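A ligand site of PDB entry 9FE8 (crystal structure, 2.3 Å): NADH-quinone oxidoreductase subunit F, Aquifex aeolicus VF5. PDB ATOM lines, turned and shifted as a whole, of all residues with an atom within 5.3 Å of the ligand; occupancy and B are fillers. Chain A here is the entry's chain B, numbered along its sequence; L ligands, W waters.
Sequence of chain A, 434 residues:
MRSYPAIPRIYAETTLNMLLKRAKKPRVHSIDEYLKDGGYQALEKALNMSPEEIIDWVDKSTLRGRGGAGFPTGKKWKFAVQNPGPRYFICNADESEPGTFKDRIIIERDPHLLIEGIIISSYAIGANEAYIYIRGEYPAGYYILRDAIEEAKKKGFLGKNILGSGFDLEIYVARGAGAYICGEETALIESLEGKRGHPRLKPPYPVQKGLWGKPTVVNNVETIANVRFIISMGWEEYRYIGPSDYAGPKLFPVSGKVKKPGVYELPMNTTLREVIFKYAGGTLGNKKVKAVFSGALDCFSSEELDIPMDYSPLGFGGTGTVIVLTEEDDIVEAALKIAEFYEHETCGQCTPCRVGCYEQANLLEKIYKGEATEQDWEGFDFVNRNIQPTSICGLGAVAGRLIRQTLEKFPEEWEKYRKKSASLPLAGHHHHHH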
ATOM      1  N   GLY A  65      21.513 -33.021 -11.879  1.00  0.00           N
ATOM      2  CA  GLY A  65      21.441 -32.225 -13.099  1.00  0.00           C
ATOM      3  C   GLY A  65      22.831 -31.940 -13.672  1.00  0.00           C
ATOM      4  O   GLY A  65      23.789 -31.767 -12.927  1.00  0.00           O
ATOM      5  N   ARG A  66      22.916 -31.898 -15.004  1.00  0.00           N
ATOM      6  CA  ARG A  66      24.166 -31.677 -15.713  1.00  0.00           C
ATOM      7  C   ARG A  66      24.214 -30.255 -16.282  1.00  0.00           C
ATOM      8  O   ARG A  66      25.103 -29.962 -17.080  1.00  0.00           O
ATOM      9  CB  ARG A  66      24.291 -32.679 -16.868  1.00  0.00           C
ATOM     10  CG  ARG A  66      24.330 -34.145 -16.470  1.00  0.00           C
ATOM     11  CD  ARG A  66      25.550 -34.489 -15.658  1.00  0.00           C
ATOM     12  NE  ARG A  66      25.632 -35.944 -15.543  1.00  0.00           N
ATOM     13  CZ  ARG A  66      25.505 -36.680 -14.438  1.00  0.00           C
ATOM     14  NH1 ARG A  66      25.801 -37.960 -14.497  1.00  0.00           N
ATOM     15  NH2 ARG A  66      25.155 -36.147 -13.280  1.00  0.00           N
ATOM     16  N   GLY A  67      23.280 -29.388 -15.866  1.00  0.00           N
ATOM     17  CA  GLY A  67      23.160 -28.047 -16.420  1.00  0.00           C
ATOM     18  C   GLY A  67      23.908 -26.978 -15.621  1.00  0.00           C
ATOM     19  O   GLY A  67      24.143 -25.885 -16.133  1.00  0.00           O
ATOM     20  N   GLY A  68      24.285 -27.328 -14.374  1.00  0.00           N
ATOM     21  CA  GLY A  68      25.225 -26.517 -13.624  1.00  0.00           C
ATOM     22  C   GLY A  68      24.836 -26.412 -12.153  1.00  0.00           C
ATOM     23  O   GLY A  68      25.708 -26.263 -11.314  1.00  0.00           O
ATOM     24  N   ALA A  69      23.531 -26.448 -11.854  1.00  0.00           N
ATOM     25  CA  ALA A  69      23.071 -26.241 -10.486  1.00  0.00           C
ATOM     26  C   ALA A  69      23.112 -27.547  -9.701  1.00  0.00           C
ATOM     27  O   ALA A  69      23.033 -27.527  -8.479  1.00  0.00           O
ATOM     28  CB  ALA A  69      21.696 -25.624 -10.478  1.00  0.00           C
ATOM     29  N   GLY A  70      23.181 -28.668 -10.425  1.00  0.00           N
ATOM     30  CA  GLY A  70      23.432 -29.988  -9.857  1.00  0.00           C
ATOM     31  C   GLY A  70      22.321 -30.480  -8.912  1.00  0.00           C
ATOM     32  O   GLY A  70      22.609 -31.171  -7.935  1.00  0.00           O
ATOM     33  N   PHE A  71      21.051 -30.174  -9.223  1.00  0.00           N
ATOM     34  CA  PHE A  71      19.964 -30.563  -8.344  1.00  0.00           C
ATOM     35  C   PHE A  71      19.592 -32.038  -8.600  1.00  0.00           C
ATOM     36  O   PHE A  71      19.459 -32.487  -9.745  1.00  0.00           O
ATOM     37  CB  PHE A  71      18.793 -29.593  -8.503  1.00  0.00           C
ATOM     38  CG  PHE A  71      17.709 -29.801  -7.446  1.00  0.00           C
ATOM     39  CD1 PHE A  71      16.736 -30.800  -7.599  1.00  0.00           C
ATOM     40  CD2 PHE A  71      17.670 -29.009  -6.303  1.00  0.00           C
ATOM     41  CE1 PHE A  71      15.760 -31.009  -6.649  1.00  0.00           C
ATOM     42  CE2 PHE A  71      16.686 -29.214  -5.339  1.00  0.00           C
ATOM     43  CZ  PHE A  71      15.732 -30.215  -5.507  1.00  0.00           C
ATOM     44  N   THR A  73      17.891 -35.229  -9.635  1.00  0.00           N
ATOM     45  CA  THR A  73      16.884 -35.232 -10.689  1.00  0.00           C
ATOM     46  C   THR A  73      15.565 -35.833 -10.224  1.00  0.00           C
ATOM     47  O   THR A  73      14.500 -35.319 -10.568  1.00  0.00           O
ATOM     48  CB  THR A  73      17.402 -36.005 -11.895  1.00  0.00           C
ATOM     49  OG1 THR A  73      18.578 -35.332 -12.341  1.00  0.00           O
ATOM     50  CG2 THR A  73      16.337 -36.049 -12.974  1.00  0.00           C
ATOM     51  N   LYS A  76      13.618 -33.589  -7.898  1.00  0.00           N
ATOM     52  CA  LYS A  76      12.959 -32.576  -8.707  1.00  0.00           C
ATOM     53  C   LYS A  76      11.652 -33.103  -9.303  1.00  0.00           C
ATOM     54  O   LYS A  76      10.612 -32.442  -9.183  1.00  0.00           O
ATOM     55  CB  LYS A  76      13.893 -32.063  -9.804  1.00  0.00           C
ATOM     56  CG  LYS A  76      13.268 -31.022 -10.707  1.00  0.00           C
ATOM     57  CD  LYS A  76      14.103 -30.679 -11.929  1.00  0.00           C
ATOM     58  CE  LYS A  76      15.450 -30.177 -11.606  1.00  0.00           C
ATOM     59  NZ  LYS A  76      16.126 -29.669 -12.807  1.00  0.00           N
ATOM     60  N   ASN A  92      16.362 -28.714 -21.943  1.00  0.00           N
ATOM     61  CA  ASN A  92      17.125 -27.488 -22.081  1.00  0.00           C
ATOM     62  C   ASN A  92      18.325 -27.765 -22.970  1.00  0.00           C
ATOM     63  O   ASN A  92      19.266 -28.429 -22.525  1.00  0.00           O
ATOM     64  CB  ASN A  92      17.518 -26.949 -20.708  1.00  0.00           C
ATOM     65  CG  ASN A  92      18.122 -25.562 -20.751  1.00  0.00           C
ATOM     66  OD1 ASN A  92      18.544 -25.082 -21.816  1.00  0.00           O
ATOM     67  ND2 ASN A  92      18.190 -24.910 -19.600  1.00  0.00           N
ATOM     68  N   ASP A  94      20.054 -25.089 -24.677  1.00  0.00           N
ATOM     69  CA  ASP A  94      20.516 -23.738 -24.995  1.00  0.00           C
ATOM     70  C   ASP A  94      22.049 -23.686 -25.021  1.00  0.00           C
ATOM     71  O   ASP A  94      22.598 -22.803 -25.674  1.00  0.00           O
ATOM     72  CB  ASP A  94      19.937 -22.696 -24.051  1.00  0.00           C
ATOM     73  CG  ASP A  94      20.009 -21.271 -24.592  1.00  0.00           C
ATOM     74  OD1 ASP A  94      19.378 -21.030 -25.656  1.00  0.00           O
ATOM     75  OD2 ASP A  94      20.692 -20.427 -23.964  1.00  0.00           O
ATOM     76  N   GLU A  95      22.711 -24.625 -24.326  1.00  0.00           N
ATOM     77  CA  GLU A  95      24.170 -24.760 -24.304  1.00  0.00           C
ATOM     78  C   GLU A  95      24.892 -23.590 -24.979  1.00  0.00           C
ATOM     79  O   GLU A  95      25.241 -23.664 -26.164  1.00  0.00           O
ATOM     80  CB  GLU A  95      24.567 -26.084 -24.977  1.00  0.00           C
ATOM     81  CG  GLU A  95      26.045 -26.399 -24.805  1.00  0.00           C
ATOM     82  CD  GLU A  95      26.422 -27.787 -25.248  1.00  0.00           C
ATOM     83  OE1 GLU A  95      26.263 -28.030 -26.469  1.00  0.00           O
ATOM     84  OE2 GLU A  95      26.864 -28.590 -24.413  1.00  0.00           O
ATOM     85  N   SER A  96      25.096 -22.493 -24.240  1.00  0.00           N
ATOM     86  CA  SER A  96      25.729 -21.297 -24.781  1.00  0.00           C
ATOM     87  C   SER A  96      26.902 -20.806 -23.926  1.00  0.00           C
ATOM     88  O   SER A  96      27.448 -19.737 -24.205  1.00  0.00           O
ATOM     89  CB  SER A  96      24.704 -20.205 -24.991  1.00  0.00           C
ATOM     90  OG  SER A  96      23.842 -20.526 -26.062  1.00  0.00           O
ATOM     91  N   ASP A 103      26.436 -31.130 -25.178  1.00  0.00           N
ATOM     92  CA  ASP A 103      25.060 -31.523 -25.426  1.00  0.00           C
ATOM     93  C   ASP A 103      24.784 -31.651 -26.918  1.00  0.00           C
ATOM     94  O   ASP A 103      23.956 -32.481 -27.310  1.00  0.00           O
ATOM     95  CB  ASP A 103      24.074 -30.531 -24.841  1.00  0.00           C
ATOM     96  CG  ASP A 103      24.136 -30.396 -23.327  1.00  0.00           C
ATOM     97  OD1 ASP A 103      24.743 -31.282 -22.679  1.00  0.00           O
ATOM     98  OD2 ASP A 103      23.614 -29.374 -22.840  1.00  0.00           O
ATOM     99  N   TYR A 180      22.197 -16.036 -24.096  1.00  0.00           N
ATOM    100  CA  TYR A 180      22.688 -17.048 -23.169  1.00  0.00           C
ATOM    101  C   TYR A 180      21.777 -17.131 -21.952  1.00  0.00           C
ATOM    102  O   TYR A 180      21.671 -18.204 -21.361  1.00  0.00           O
ATOM    103  CB  TYR A 180      24.102 -16.714 -22.712  1.00  0.00           C
ATOM    104  CG  TYR A 180      24.614 -17.433 -21.464  1.00  0.00           C
ATOM    105  CD1 TYR A 180      25.040 -18.751 -21.518  1.00  0.00           C
ATOM    106  CD2 TYR A 180      24.739 -16.762 -20.254  1.00  0.00           C
ATOM    107  CE1 TYR A 180      25.563 -19.397 -20.409  1.00  0.00           C
ATOM    108  CE2 TYR A 180      25.242 -17.405 -19.129  1.00  0.00           C
ATOM    109  CZ  TYR A 180      25.645 -18.721 -19.199  1.00  0.00           C
ATOM    110  OH  TYR A 180      26.145 -19.364 -18.106  1.00  0.00           O
ATOM    111  N   ILE A 181      21.123 -16.023 -21.572  1.00  0.00           N
ATOM    112  CA  ILE A 181      20.298 -16.033 -20.380  1.00  0.00           C
ATOM    113  C   ILE A 181      19.107 -16.981 -20.571  1.00  0.00           C
ATOM    114  O   ILE A 181      18.540 -17.452 -19.583  1.00  0.00           O
ATOM    115  CB  ILE A 181      19.859 -14.607 -19.976  1.00  0.00           C
ATOM    116  CG1 ILE A 181      19.288 -14.557 -18.564  1.00  0.00           C
ATOM    117  CG2 ILE A 181      18.867 -14.020 -20.995  1.00  0.00           C
ATOM    118  CD1 ILE A 181      20.216 -15.079 -17.479  1.00  0.00           C
ATOM    119  N   GLY A 183      19.188 -19.925 -21.344  1.00  0.00           N
ATOM    120  CA  GLY A 183      19.503 -21.178 -20.669  1.00  0.00           C
ATOM    121  C   GLY A 183      19.017 -21.231 -19.211  1.00  0.00           C
ATOM    122  O   GLY A 183      18.816 -22.306 -18.646  1.00  0.00           O
ATOM    123  N   GLU A 184      18.855 -20.055 -18.580  1.00  0.00           N
ATOM    124  CA  GLU A 184      18.351 -20.012 -17.216  1.00  0.00           C
ATOM    125  C   GLU A 184      16.889 -20.434 -17.296  1.00  0.00           C
ATOM    126  O   GLU A 184      16.146 -19.876 -18.093  1.00  0.00           O
ATOM    127  CB  GLU A 184      18.586 -18.621 -16.629  1.00  0.00           C
ATOM    128  CG  GLU A 184      18.417 -18.569 -15.111  1.00  0.00           C
ATOM    129  CD  GLU A 184      16.985 -18.427 -14.610  1.00  0.00           C
ATOM    130  OE1 GLU A 184      16.064 -18.146 -15.413  1.00  0.00           O
ATOM    131  OE2 GLU A 184      16.796 -18.609 -13.403  1.00  0.00           O
ATOM    132  N   GLU A 185      16.512 -21.443 -16.504  1.00  0.00           N
ATOM    133  CA  GLU A 185      15.225 -22.139 -16.624  1.00  0.00           C
ATOM    134  C   GLU A 185      14.019 -21.181 -16.673  1.00  0.00           C
ATOM    135  O   GLU A 185      13.125 -21.418 -17.485  1.00  0.00           O
ATOM    136  CB  GLU A 185      15.083 -23.230 -15.550  1.00  0.00           C
ATOM    137  CG  GLU A 185      15.336 -22.775 -14.115  1.00  0.00           C
ATOM    138  CD  GLU A 185      14.967 -23.783 -13.024  1.00  0.00           C
ATOM    139  OE1 GLU A 185      14.497 -24.874 -13.368  1.00  0.00           O
ATOM    140  OE2 GLU A 185      15.130 -23.453 -11.807  1.00  0.00           O
ATOM    141  N   VAL A 218      12.318 -28.750 -15.904  1.00  0.00           N
ATOM    142  CA  VAL A 218      13.336 -28.459 -16.889  1.00  0.00           C
ATOM    143  C   VAL A 218      14.560 -29.312 -16.561  1.00  0.00           C
ATOM    144  O   VAL A 218      15.047 -29.262 -15.435  1.00  0.00           O
ATOM    145  CB  VAL A 218      13.662 -26.957 -16.872  1.00  0.00           C
ATOM    146  CG1 VAL A 218      14.765 -26.623 -17.858  1.00  0.00           C
ATOM    147  CG2 VAL A 218      12.424 -26.095 -17.140  1.00  0.00           C
ATOM    148  N   ASN A 219      15.032 -30.112 -17.532  1.00  0.00           N
ATOM    149  CA  ASN A 219      16.267 -30.860 -17.374  1.00  0.00           C
ATOM    150  C   ASN A 219      17.174 -30.560 -18.570  1.00  0.00           C
ATOM    151  O   ASN A 219      16.659 -30.311 -19.675  1.00  0.00           O
ATOM    152  CB  ASN A 219      16.014 -32.354 -17.209  1.00  0.00           C
ATOM    153  CG  ASN A 219      15.645 -32.760 -15.797  1.00  0.00           C
ATOM    154  OD1 ASN A 219      14.590 -33.349 -15.571  1.00  0.00           O
ATOM    155  ND2 ASN A 219      16.521 -32.476 -14.826  1.00  0.00           N
ATOM    156  N   ASN A 220      18.496 -30.615 -18.313  1.00  0.00           N
ATOM    157  CA  ASN A 220      19.539 -30.492 -19.327  1.00  0.00           C
ATOM    158  C   ASN A 220      19.570 -31.727 -20.254  1.00  0.00           C
ATOM    159  O   ASN A 220      19.285 -32.829 -19.821  1.00  0.00           O
ATOM    160  CB  ASN A 220      20.896 -30.269 -18.672  1.00  0.00           C
ATOM    161  CG  ASN A 220      22.037 -30.162 -19.667  1.00  0.00           C
ATOM    162  OD1 ASN A 220      22.065 -29.216 -20.468  1.00  0.00           O
ATOM    163  ND2 ASN A 220      22.970 -31.096 -19.633  1.00  0.00           N
ATOM    164  N   VAL A 221      19.942 -31.529 -21.533  1.00  0.00           N
ATOM    165  CA  VAL A 221      20.070 -32.595 -22.507  1.00  0.00           C
ATOM    166  C   VAL A 221      20.780 -33.815 -21.906  1.00  0.00           C
ATOM    167  O   VAL A 221      20.248 -34.915 -21.951  1.00  0.00           O
ATOM    168  CB  VAL A 221      20.829 -32.133 -23.760  1.00  0.00           C
ATOM    169  CG1 VAL A 221      21.258 -33.309 -24.624  1.00  0.00           C
ATOM    170  CG2 VAL A 221      20.020 -31.139 -24.569  1.00  0.00           C
ATOM    171  N   THR A 223      21.379 -34.659 -18.830  1.00  0.00           N
ATOM    172  CA  THR A 223      20.626 -35.277 -17.738  1.00  0.00           C
ATOM    173  C   THR A 223      19.656 -36.309 -18.300  1.00  0.00           C
ATOM    174  O   THR A 223      19.609 -37.443 -17.816  1.00  0.00           O
ATOM    175  CB  THR A 223      19.896 -34.222 -16.912  1.00  0.00           C
ATOM    176  OG1 THR A 223      20.821 -33.160 -16.653  1.00  0.00           O
ATOM    177  CG2 THR A 223      19.403 -34.804 -15.589  1.00  0.00           C
ATOM    178  N   CYS A 393      18.915 -13.877 -10.501  1.00  0.00           N
ATOM    179  CA  CYS A 393      19.336 -15.110 -11.179  1.00  0.00           C
ATOM    180  C   CYS A 393      20.839 -15.264 -11.001  1.00  0.00           C
ATOM    181  O   CYS A 393      21.486 -14.353 -10.483  1.00  0.00           O
ATOM    182  CB  CYS A 393      18.918 -15.166 -12.652  1.00  0.00           C
ATOM    183  SG  CYS A 393      20.186 -14.663 -13.870  1.00  0.00           S
ATOM    184  N   GLY A 394      21.391 -16.405 -11.415  1.00  0.00           N
ATOM    185  CA  GLY A 394      22.753 -16.799 -11.066  1.00  0.00           C
ATOM    186  C   GLY A 394      23.833 -16.109 -11.917  1.00  0.00           C
ATOM    187  O   GLY A 394      24.985 -16.078 -11.513  1.00  0.00           O
ATOM    188  N   LEU A 395      23.448 -15.526 -13.073  1.00  0.00           N
ATOM    189  CA  LEU A 395      24.391 -14.805 -13.909  1.00  0.00           C
ATOM    190  C   LEU A 395      25.051 -13.697 -13.102  1.00  0.00           C
ATOM    191  O   LEU A 395      26.265 -13.522 -13.133  1.00  0.00           O
ATOM    192  CB  LEU A 395      23.721 -14.245 -15.158  1.00  0.00           C
ATOM    193  CG  LEU A 395      24.680 -13.738 -16.230  1.00  0.00           C
ATOM    194  CD1 LEU A 395      24.065 -13.844 -17.630  1.00  0.00           C
ATOM    195  CD2 LEU A 395      25.106 -12.312 -15.937  1.00  0.00           C
HETATM  196  C1  LIG L   1      21.675 -21.966 -16.756  1.00  0.00           C
HETATM  197  N1  LIG L   1      21.308 -23.326 -16.824  1.00  0.00           N
HETATM  198  C2  LIG L   1      21.434 -24.006 -18.010  1.00  0.00           C
HETATM  199  N2  LIG L   1      21.030 -25.305 -18.051  1.00  0.00           N
HETATM  200  C3  LIG L   1      21.051 -26.049 -19.185  1.00  0.00           C
HETATM  201  O1  LIG L   1      20.597 -27.184 -19.225  1.00  0.00           O
HETATM  202  N3  LIG L   1      21.565 -25.423 -20.294  1.00  0.00           N
HETATM  203  C4  LIG L   1      22.025 -24.124 -20.382  1.00  0.00           C
HETATM  204  O2  LIG L   1      22.482 -23.718 -21.435  1.00  0.00           O
HETATM  205  C5  LIG L   1      21.926 -23.392 -19.151  1.00  0.00           C
HETATM  206  N4  LIG L   1      22.289 -22.087 -19.111  1.00  0.00           N
HETATM  207  C6  LIG L   1      22.152 -21.345 -17.923  1.00  0.00           C
HETATM  208  C7  LIG L   1      22.505 -19.993 -17.898  1.00  0.00           C
HETATM  209  C8  LIG L   1      22.377 -19.255 -16.724  1.00  0.00           C
HETATM  210  C9  LIG L   1      22.803 -17.804 -16.712  1.00  0.00           C
HETATM  211  C10 LIG L   1      21.902 -19.886 -15.561  1.00  0.00           C
HETATM  212  C11 LIG L   1      21.822 -19.140 -14.243  1.00  0.00           C
HETATM  213  C12 LIG L   1      21.556 -21.224 -15.593  1.00  0.00           C
HETATM  214  C13 LIG L   1      20.753 -24.015 -15.644  1.00  0.00           C
HETATM  215  C14 LIG L   1      19.233 -24.095 -15.715  1.00  0.00           C
HETATM  216  O3  LIG L   1      18.678 -22.897 -15.163  1.00  0.00           O
HETATM  217  C15 LIG L   1      18.748 -25.317 -14.932  1.00  0.00           C
HETATM  218  O4  LIG L   1      19.493 -25.455 -13.726  1.00  0.00           O
HETATM  219  C16 LIG L   1      18.886 -26.637 -15.704  1.00  0.00           C
HETATM  220  O5  LIG L   1      18.529 -26.505 -17.082  1.00  0.00           O
HETATM  221  C17 LIG L   1      18.089 -27.723 -15.019  1.00  0.00           C
HETATM  222  O6  LIG L   1      18.381 -28.986 -15.630  1.00  0.00           O
HETATM  223  P1  LIG L   1      19.269 -30.063 -14.799  1.00  0.00           P
HETATM  224  O7  LIG L   1      19.124 -31.307 -15.674  1.00  0.00           O
HETATM  225  O8  LIG L   1      18.614 -30.219 -13.441  1.00  0.00           O
HETATM  226  O9  LIG L   1      20.689 -29.565 -14.707  1.00  0.00           O
HETATM  227  O   HOH W   1      25.057 -23.148 -21.258  1.00  0.00           O
HETATM  228  O   HOH W   2      22.792 -20.849 -22.391  1.00  0.00           O
HETATM  229  O   HOH W   3      20.245 -28.873 -11.473  1.00  0.00           O
HETATM  230  O   HOH W   4      19.529 -21.890 -12.411  1.00  0.00           O
HETATM  231  O   HOH W   5      18.247 -32.520 -12.090  1.00  0.00           O
HETATM  232  O   HOH W   6      21.645 -27.248 -22.801  1.00  0.00           O
HETATM  233  O   HOH W   7      21.364 -27.495 -13.535  1.00  0.00           O
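O8 of the ligand is in salt-bridge range of NZ of Lys 76, at 2.6 Å. OG1 of Thr 223 is in hydrogen-bond range of O7 of the ligand (2.7 Å). N of Asn 220 sits at hydrogen-bond distance from O7 of the ligand, 2.8 Å away. The side-chain amide oxygen (OD1) of Asn 220 lies close to an oxygen (O1) of the ligand. O9 of the ligand is in hydrogen-bond range of N of Gly 67. The backbone NH (N) of Glu 185 is in hydrogen-bond range of an oxygen (O3) of the ligand, at 2.9 Å. An oxygen (O7) of the ligand lies within hydrogen-bond range of the side-chain amide nitrogen of Asn 219. The side-chain amide nitrogen (ND2) of Asn 92 is in hydrogen-bond range of an oxygen (O5) of the ligand, at 3.0 Å. N of Glu 95 lies within hydrogen-bond range of O2 of the ligand (3.0 Å). N of Arg 66 sits at hydrogen-bond distance from O9 of the ligand, 3.2 Å away.
ND2 of Asn 219 lies close to NZ of Lys 76, 3.5 Å away. The side-chain hydroxyl (OG1) of Thr 223 lies within hydrogen-bond range of the backbone NH (N) of Arg 66, 2.9 Å away. The side-chain amide oxygen (OD1) of Asn 220 sits close to the side-chain carboxylate (OD2) of Asp 103. N of Asn 92 is in hydrogen-bond range of O of Asn 219 (2.8 Å). N of Asp 94 lies within hydrogen-bond range of OD1 of Asn 92 (3.2 Å). N of Gly 183 sits at hydrogen-bond distance from OD2 of Asp 94, 3.1 Å away. O of Phe 71 sits at hydrogen-bond distance from N of Gly 65, 3.0 Å away. N of Leu 395 sits close to SG of Cys 393 (3.5 Å).
O of Gly 183 lies close to N1 of the ligand, 3.3 Å away. The backbone carbonyl oxygen (O) of Val 218 lies close to an oxygen (O6) of the ligand (3.4 Å). CA of Gly 65 touches O9 of the ligand, 3.2 Å away. Ala 69 touches the ligand. Asp 94 touches the ligand (C to O2, 3.6 Å). CE2 of Tyr 180 touches C9 of the ligand, 3.5 Å away. CD1 of Ile 181 touches C9 of the ligand, 3.8 Å away. CA of Glu 184 touches O3 of the ligand, 3.6 Å away. N of Gly 394 touches C11 of the ligand (3.96 Å). Leu 395 touches the ligand. Of the 27 residues printed, 19 come within 4 Å of the ligand.
Water W7 lies within hydrogen-bond range of an oxygen (O9) of the ligand, the backbone NH (N) of Ala 69 and the backbone NH (N) of Gly 68. Water W1 bridges O2 of the ligand (2.6 Å) and N of Ser 96 (3.1 Å). Water W5 lies within hydrogen-bond range of the backbone carbonyl oxygen of Phe 71 (2.6 Å), an oxygen (O8) of the ligand (2.7 Å), the side-chain hydroxyl of Thr 73 (2.8 Å), the side-chain amide nitrogen of Asn 219 (3.2 Å) and the backbone NH of Gly 65 (3.3 Å). Water W3 lies within hydrogen-bond range of N of Phe 71 (2.7 Å), O8 of the ligand (2.9 Å) and N of Gly 70 (3.1 Å).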
